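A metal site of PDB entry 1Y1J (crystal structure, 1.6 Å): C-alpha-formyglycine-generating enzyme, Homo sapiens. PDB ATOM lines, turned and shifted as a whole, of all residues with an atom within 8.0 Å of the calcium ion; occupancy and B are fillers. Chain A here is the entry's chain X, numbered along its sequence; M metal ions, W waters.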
ATOM      1  N   TYR A  57      25.960  12.440 -19.159  1.00  0.00           N
ATOM      2  CA  TYR A  57      25.871  11.438 -18.128  1.00  0.00           C
ATOM      3  C   TYR A  57      27.217  11.269 -17.396  1.00  0.00           C
ATOM      4  O   TYR A  57      28.295  11.438 -17.974  1.00  0.00           O
ATOM      5  CB  TYR A  57      25.551  10.070 -18.747  1.00  0.00           C
ATOM      6  CG  TYR A  57      24.388  10.046 -19.718  1.00  0.00           C
ATOM      7  CD1 TYR A  57      23.097  10.238 -19.279  1.00  0.00           C
ATOM      8  CD2 TYR A  57      24.603   9.880 -21.076  1.00  0.00           C
ATOM      9  CE1 TYR A  57      22.040  10.246 -20.155  1.00  0.00           C
ATOM     10  CE2 TYR A  57      23.547   9.867 -21.965  1.00  0.00           C
ATOM     11  CZ  TYR A  57      22.269  10.037 -21.503  1.00  0.00           C
ATOM     12  OH  TYR A  57      21.193  10.042 -22.367  1.00  0.00           O
ATOM     13  N   GLU A  58      27.132  10.858 -16.141  1.00  0.00           N
ATOM     14  CA  GLU A  58      28.284  10.329 -15.444  1.00  0.00           C
ATOM     15  C   GLU A  58      28.831   9.181 -16.309  1.00  0.00           C
ATOM     16  O   GLU A  58      28.066   8.512 -17.017  1.00  0.00           O
ATOM     17  CB  GLU A  58      27.883   9.779 -14.080  1.00  0.00           C
ATOM     18  CG  GLU A  58      27.312  10.806 -13.127  1.00  0.00           C
ATOM     19  CD  GLU A  58      26.382  10.225 -12.080  1.00  0.00           C
ATOM     20  OE1 GLU A  58      25.599   9.321 -12.402  1.00  0.00           O
ATOM     21  OE2 GLU A  58      26.389  10.701 -10.921  1.00  0.00           O
ATOM     22  N   PRO A 133      26.903   4.536 -12.797  1.00  0.00           N
ATOM     23  CA  PRO A 133      28.174   5.255 -12.816  1.00  0.00           C
ATOM     24  C   PRO A 133      29.342   4.387 -12.324  1.00  0.00           C
ATOM     25  O   PRO A 133      29.180   3.602 -11.387  1.00  0.00           O
ATOM     26  CB  PRO A 133      27.949   6.415 -11.848  1.00  0.00           C
ATOM     27  CG  PRO A 133      26.822   5.994 -10.990  1.00  0.00           C
ATOM     28  CD  PRO A 133      25.942   5.157 -11.877  1.00  0.00           C
ATOM     29  N   TRP A 159      31.821  23.036 -14.216  1.00  0.00           N
ATOM     30  CA  TRP A 159      30.930  22.038 -13.627  1.00  0.00           C
ATOM     31  C   TRP A 159      29.744  22.741 -12.986  1.00  0.00           C
ATOM     32  O   TRP A 159      28.576  22.361 -13.245  1.00  0.00           O
ATOM     33  CB  TRP A 159      31.687  21.143 -12.625  1.00  0.00           C
ATOM     34  CG  TRP A 159      30.851  20.008 -12.153  1.00  0.00           C
ATOM     35  CD1 TRP A 159      30.935  18.697 -12.555  1.00  0.00           C
ATOM     36  CD2 TRP A 159      29.813  20.052 -11.171  1.00  0.00           C
ATOM     37  NE1 TRP A 159      30.004  17.928 -11.910  1.00  0.00           N
ATOM     38  CE2 TRP A 159      29.301  18.738 -11.051  1.00  0.00           C
ATOM     39  CE3 TRP A 159      29.243  21.068 -10.401  1.00  0.00           C
ATOM     40  CZ2 TRP A 159      28.244  18.432 -10.206  1.00  0.00           C
ATOM     41  CZ3 TRP A 159      28.182  20.748  -9.557  1.00  0.00           C
ATOM     42  CH2 TRP A 159      27.712  19.433  -9.472  1.00  0.00           C
ATOM     43  N   ASN A 187      18.987  11.259  -7.153  1.00  0.00           N
ATOM     44  CA  ASN A 187      19.203  10.089  -6.310  1.00  0.00           C
ATOM     45  C   ASN A 187      20.053  10.471  -5.097  1.00  0.00           C
ATOM     46  O   ASN A 187      21.238  10.549  -5.192  1.00  0.00           O
ATOM     47  CB  ASN A 187      19.890   8.958  -7.098  1.00  0.00           C
ATOM     48  CG  ASN A 187      20.112   7.710  -6.242  1.00  0.00           C
ATOM     49  OD1 ASN A 187      19.453   7.562  -5.212  1.00  0.00           O
ATOM     50  ND2 ASN A 187      21.020   6.794  -6.672  1.00  0.00           N
ATOM     51  N   TYR A 220      22.154  14.841 -16.778  1.00  0.00           N
ATOM     52  CA  TYR A 220      21.507  13.888 -15.891  1.00  0.00           C
ATOM     53  C   TYR A 220      22.381  13.645 -14.663  1.00  0.00           C
ATOM     54  O   TYR A 220      23.601  13.540 -14.803  1.00  0.00           O
ATOM     55  CB  TYR A 220      21.303  12.540 -16.600  1.00  0.00           C
ATOM     56  CG  TYR A 220      20.327  12.598 -17.759  1.00  0.00           C
ATOM     57  CD1 TYR A 220      20.691  13.123 -18.990  1.00  0.00           C
ATOM     58  CD2 TYR A 220      19.014  12.150 -17.593  1.00  0.00           C
ATOM     59  CE1 TYR A 220      19.801  13.192 -20.000  1.00  0.00           C
ATOM     60  CE2 TYR A 220      18.116  12.208 -18.618  1.00  0.00           C
ATOM     61  CZ  TYR A 220      18.505  12.723 -19.829  1.00  0.00           C
ATOM     62  OH  TYR A 220      17.631  12.800 -20.894  1.00  0.00           O
ATOM     63  N   ASN A 221      21.749  13.578 -13.491  1.00  0.00           N
ATOM     64  CA  ASN A 221      22.420  13.193 -12.239  1.00  0.00           C
ATOM     65  C   ASN A 221      23.628  14.026 -11.890  1.00  0.00           C
ATOM     66  O   ASN A 221      24.601  13.532 -11.300  1.00  0.00           O
ATOM     67  CB  ASN A 221      22.754  11.718 -12.289  1.00  0.00           C
ATOM     68  CG  ASN A 221      21.508  10.874 -12.421  1.00  0.00           C
ATOM     69  OD1 ASN A 221      20.650  10.896 -11.533  1.00  0.00           O
ATOM     70  ND2 ASN A 221      21.357  10.185 -13.550  1.00  0.00           N
ATOM     71  N   ILE A 222      23.572  15.305 -12.249  1.00  0.00           N
ATOM     72  CA  ILE A 222      24.692  16.207 -11.958  1.00  0.00           C
ATOM     73  C   ILE A 222      24.686  16.550 -10.476  1.00  0.00           C
ATOM     74  O   ILE A 222      25.748  16.767  -9.918  1.00  0.00           O
ATOM     75  CB  ILE A 222      24.726  17.440 -12.914  1.00  0.00           C
ATOM     76  CG1 ILE A 222      26.044  18.215 -12.741  1.00  0.00           C
ATOM     77  CG2 ILE A 222      23.527  18.306 -12.724  1.00  0.00           C
ATOM     78  CD1 ILE A 222      26.669  18.654 -13.967  1.00  0.00           C
ATOM     79  N   VAL A 223      23.531  16.559  -9.812  1.00  0.00           N
ATOM     80  CA  VAL A 223      23.508  16.396  -8.340  1.00  0.00           C
ATOM     81  C   VAL A 223      23.027  14.982  -7.986  1.00  0.00           C
ATOM     82  O   VAL A 223      22.207  14.360  -8.700  1.00  0.00           O
ATOM     83  CB  VAL A 223      22.689  17.462  -7.540  1.00  0.00           C
ATOM     84  CG1 VAL A 223      23.283  18.855  -7.737  1.00  0.00           C
ATOM     85  CG2 VAL A 223      21.223  17.429  -7.857  1.00  0.00           C
ATOM     86  N   GLY A 224      23.600  14.431  -6.925  1.00  0.00           N
ATOM     87  CA  GLY A 224      23.291  13.075  -6.557  1.00  0.00           C
ATOM     88  C   GLY A 224      23.916  11.975  -7.390  1.00  0.00           C
ATOM     89  O   GLY A 224      24.681  12.225  -8.348  1.00  0.00           O
ATOM     90  N   ASN A 225      23.581  10.744  -7.005  1.00  0.00           N
ATOM     91  CA  ASN A 225      24.019   9.499  -7.632  1.00  0.00           C
ATOM     92  C   ASN A 225      25.493   9.286  -7.260  1.00  0.00           C
ATOM     93  O   ASN A 225      25.754   8.825  -6.166  1.00  0.00           O
ATOM     94  CB  ASN A 225      23.714   9.452  -9.139  1.00  0.00           C
ATOM     95  CG  ASN A 225      23.388   8.058  -9.627  1.00  0.00           C
ATOM     96  OD1 ASN A 225      22.802   7.272  -8.882  1.00  0.00           O
ATOM     97  ND2 ASN A 225      23.727   7.741 -10.885  1.00  0.00           N
ATOM     98  N   ALA A 226      26.447   9.648  -8.131  1.00  0.00           N
ATOM     99  CA  ALA A 226      27.861   9.661  -7.758  1.00  0.00           C
ATOM    100  C   ALA A 226      28.339  11.123  -7.646  1.00  0.00           C
ATOM    101  O   ALA A 226      27.916  12.007  -8.425  1.00  0.00           O
ATOM    102  CB  ALA A 226      28.692   8.926  -8.782  1.00  0.00           C
ATOM    103  N   TRP A 227      29.208  11.375  -6.658  1.00  0.00           N
ATOM    104  CA  TRP A 227      30.043  12.585  -6.645  1.00  0.00           C
ATOM    105  C   TRP A 227      30.825  12.672  -7.938  1.00  0.00           C
ATOM    106  O   TRP A 227      31.075  11.634  -8.576  1.00  0.00           O
ATOM    107  CB  TRP A 227      31.074  12.536  -5.522  1.00  0.00           C
ATOM    108  CG  TRP A 227      30.599  12.938  -4.186  1.00  0.00           C
ATOM    109  CD1 TRP A 227      30.157  12.127  -3.189  1.00  0.00           C
ATOM    110  CD2 TRP A 227      30.521  14.286  -3.666  1.00  0.00           C
ATOM    111  NE1 TRP A 227      29.832  12.870  -2.062  1.00  0.00           N
ATOM    112  CE2 TRP A 227      30.034  14.204  -2.343  1.00  0.00           C
ATOM    113  CE3 TRP A 227      30.863  15.544  -4.182  1.00  0.00           C
ATOM    114  CZ2 TRP A 227      29.881  15.323  -1.546  1.00  0.00           C
ATOM    115  CZ3 TRP A 227      30.656  16.672  -3.389  1.00  0.00           C
ATOM    116  CH2 TRP A 227      30.193  16.548  -2.090  1.00  0.00           C
ATOM    117  N   GLU A 228      31.275  13.880  -8.286  1.00  0.00           N
ATOM    118  CA  GLU A 228      31.963  14.083  -9.560  1.00  0.00           C
ATOM    119  C   GLU A 228      33.250  14.883  -9.404  1.00  0.00           C
ATOM    120  O   GLU A 228      33.262  16.009  -8.930  1.00  0.00           O
ATOM    121  CB  GLU A 228      31.012  14.740 -10.567  1.00  0.00           C
ATOM    122  CG  GLU A 228      29.746  13.898 -10.662  1.00  0.00           C
ATOM    123  CD  GLU A 228      28.746  14.394 -11.686  1.00  0.00           C
ATOM    124  OE1 GLU A 228      29.067  15.285 -12.461  1.00  0.00           O
ATOM    125  OE2 GLU A 228      27.596  13.908 -11.619  1.00  0.00           O
ATOM    126  N   LYS A 258      32.306  17.607  -6.731  1.00  0.00           N
ATOM    127  CA  LYS A 258      31.044  18.347  -6.727  1.00  0.00           C
ATOM    128  C   LYS A 258      29.833  17.421  -6.817  1.00  0.00           C
ATOM    129  O   LYS A 258      29.905  16.313  -7.350  1.00  0.00           O
ATOM    130  CB  LYS A 258      30.980  19.329  -7.905  1.00  0.00           C
ATOM    131  CG  LYS A 258      32.053  20.396  -7.912  1.00  0.00           C
ATOM    132  CD  LYS A 258      31.769  21.559  -6.957  1.00  0.00           C
ATOM    133  CE  LYS A 258      30.859  22.609  -7.571  1.00  0.00           C
ATOM    134  NZ  LYS A 258      30.700  23.803  -6.623  1.00  0.00           N
ATOM    135  N   GLY A 259      28.706  17.962  -6.359  1.00  0.00           N
ATOM    136  CA  GLY A 259      27.407  17.421  -6.687  1.00  0.00           C
ATOM    137  C   GLY A 259      26.724  16.470  -5.714  1.00  0.00           C
ATOM    138  O   GLY A 259      25.530  16.228  -5.872  1.00  0.00           O
ATOM    139  N   GLY A 260      27.441  15.915  -4.740  1.00  0.00           N
ATOM    140  CA  GLY A 260      26.811  14.962  -3.836  1.00  0.00           C
ATOM    141  C   GLY A 260      26.501  13.641  -4.493  1.00  0.00           C
ATOM    142  O   GLY A 260      26.748  13.470  -5.689  1.00  0.00           O
ATOM    143  N   SER A 261      26.019  12.705  -3.680  1.00  0.00           N
ATOM    144  CA  SER A 261      25.830  11.326  -4.062  1.00  0.00           C
ATOM    145  C   SER A 261      24.527  10.753  -3.512  1.00  0.00           C
ATOM    146  O   SER A 261      23.786  11.433  -2.794  1.00  0.00           O
ATOM    147  CB  SER A 261      26.995  10.500  -3.547  1.00  0.00           C
ATOM    148  OG  SER A 261      26.880  10.238  -2.142  1.00  0.00           O
ATOM    149  N   TYR A 262      24.296   9.482  -3.816  1.00  0.00           N
ATOM    150  CA  TYR A 262      23.145   8.736  -3.261  1.00  0.00           C
ATOM    151  C   TYR A 262      23.077   8.671  -1.742  1.00  0.00           C
ATOM    152  O   TYR A 262      22.037   8.255  -1.178  1.00  0.00           O
ATOM    153  CB  TYR A 262      23.107   7.326  -3.849  1.00  0.00           C
ATOM    154  CG  TYR A 262      24.189   6.367  -3.380  1.00  0.00           C
ATOM    155  CD1 TYR A 262      25.325   6.093  -4.149  1.00  0.00           C
ATOM    156  CD2 TYR A 262      24.016   5.678  -2.197  1.00  0.00           C
ATOM    157  CE1 TYR A 262      26.259   5.180  -3.703  1.00  0.00           C
ATOM    158  CE2 TYR A 262      24.945   4.781  -1.746  1.00  0.00           C
ATOM    159  CZ  TYR A 262      26.061   4.534  -2.497  1.00  0.00           C
ATOM    160  OH  TYR A 262      26.952   3.599  -2.065  1.00  0.00           O
ATOM    161  N   ASN A 288      31.115   6.036  -3.652  1.00  0.00           N
ATOM    162  CA  ASN A 288      30.121   7.070  -4.020  1.00  0.00           C
ATOM    163  C   ASN A 288      30.690   8.200  -4.888  1.00  0.00           C
ATOM    164  O   ASN A 288      30.082   9.250  -5.028  1.00  0.00           O
ATOM    165  CB  ASN A 288      29.536   7.683  -2.754  1.00  0.00           C
ATOM    166  CG  ASN A 288      30.530   8.553  -2.006  1.00  0.00           C
ATOM    167  OD1 ASN A 288      31.730   8.521  -2.230  1.00  0.00           O
ATOM    168  ND2 ASN A 288      29.997   9.370  -1.067  1.00  0.00           N
ATOM    169  N   GLY A 290      32.467   9.252  -8.589  1.00  0.00           N
ATOM    170  CA  GLY A 290      32.713   9.031 -10.004  1.00  0.00           C
ATOM    171  C   GLY A 290      33.107  10.336 -10.691  1.00  0.00           C
ATOM    172  O   GLY A 290      33.788  11.184 -10.111  1.00  0.00           O
ATOM    173  N   PHE A 291      32.694  10.473 -11.952  1.00  0.00           N
ATOM    174  CA  PHE A 291      33.016  11.632 -12.736  1.00  0.00           C
ATOM    175  C   PHE A 291      32.302  11.646 -14.084  1.00  0.00           C
ATOM    176  O   PHE A 291      31.748  10.649 -14.526  1.00  0.00           O
ATOM    177  CB  PHE A 291      34.521  11.716 -13.019  1.00  0.00           C
ATOM    178  CG  PHE A 291      35.031  10.617 -13.900  1.00  0.00           C
ATOM    179  CD1 PHE A 291      35.339  10.879 -15.219  1.00  0.00           C
ATOM    180  CD2 PHE A 291      35.181   9.335 -13.426  1.00  0.00           C
ATOM    181  CE1 PHE A 291      35.818   9.881 -16.049  1.00  0.00           C
ATOM    182  CE2 PHE A 291      35.650   8.332 -14.247  1.00  0.00           C
ATOM    183  CZ  PHE A 291      35.988   8.605 -15.550  1.00  0.00           C
ATOM    184  N   ARG A 292      32.329  12.831 -14.702  1.00  0.00           N
ATOM    185  CA  ARG A 292      31.977  12.997 -16.125  1.00  0.00           C
ATOM    186  C   ARG A 292      33.048  13.871 -16.761  1.00  0.00           C
ATOM    187  O   ARG A 292      33.763  14.594 -16.080  1.00  0.00           O
ATOM    188  CB  ARG A 292      30.594  13.638 -16.307  1.00  0.00           C
ATOM    189  CG  ARG A 292      30.508  15.128 -16.049  1.00  0.00           C
ATOM    190  CD  ARG A 292      29.072  15.639 -16.188  1.00  0.00           C
ATOM    191  NE  ARG A 292      28.216  15.116 -15.129  1.00  0.00           N
ATOM    192  CZ  ARG A 292      26.965  14.669 -15.295  1.00  0.00           C
ATOM    193  NH1 ARG A 292      26.395  14.661 -16.487  1.00  0.00           N
ATOM    194  NH2 ARG A 292      26.290  14.218 -14.237  1.00  0.00           N
HETATM  195 CA    CA M   1      26.370  12.792  -9.938  1.00  0.00          CA
HETATM  196  O   HOH W   1      26.779  14.595  -8.431  1.00  0.00           O
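O of Ala 226 is bound to the calcium ion, at 2.3 Å.
The calcium ion is bound by OE2 of Glu 58, 2.3 Å away.
The backbone carbonyl oxygen (O) of Asn 221 is bound to the calcium ion, at 2.4 Å.
The calcium ion is bound by the side-chain carboxylate (OE2) of Glu 228, at 2.4 Å.
The calcium ion is bound by water W1 (2.4 Å).
The backbone carbonyl oxygen (O) of Gly 224 binds the calcium ion (2.4 Å).
The calcium ion has six donor atoms within binding distance.
Five residues have an atom within 4 Å of the calcium ion: Glu 58, Asn 221, Gly 224, Ala 226 and Glu 228.
Along chain A the residues within 4 Å of the calcium ion span positions 58 to 228.
The backbone carbonyl oxygen of Asn 221 sits close to the guanidinium group of Arg 292 (3.5 Å).
The backbone NH of Gly 224 sits at hydrogen-bond distance from the backbone carbonyl oxygen of Gly 259 (2.8 Å).
OE1 of Glu 228 is in salt-bridge range of NE of Arg 292.
OE1 of Glu 228 sits at hydrogen-bond distance from NE1 of Trp 159 (2.9 Å).
The backbone carbonyl oxygen (O) of Glu 228 is in hydrogen-bond range of the backbone NH (N) of Lys 258 (2.9 Å).
OE1 of Glu 58 sits at hydrogen-bond distance from ND2 of Asn 225 (2.9 Å).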
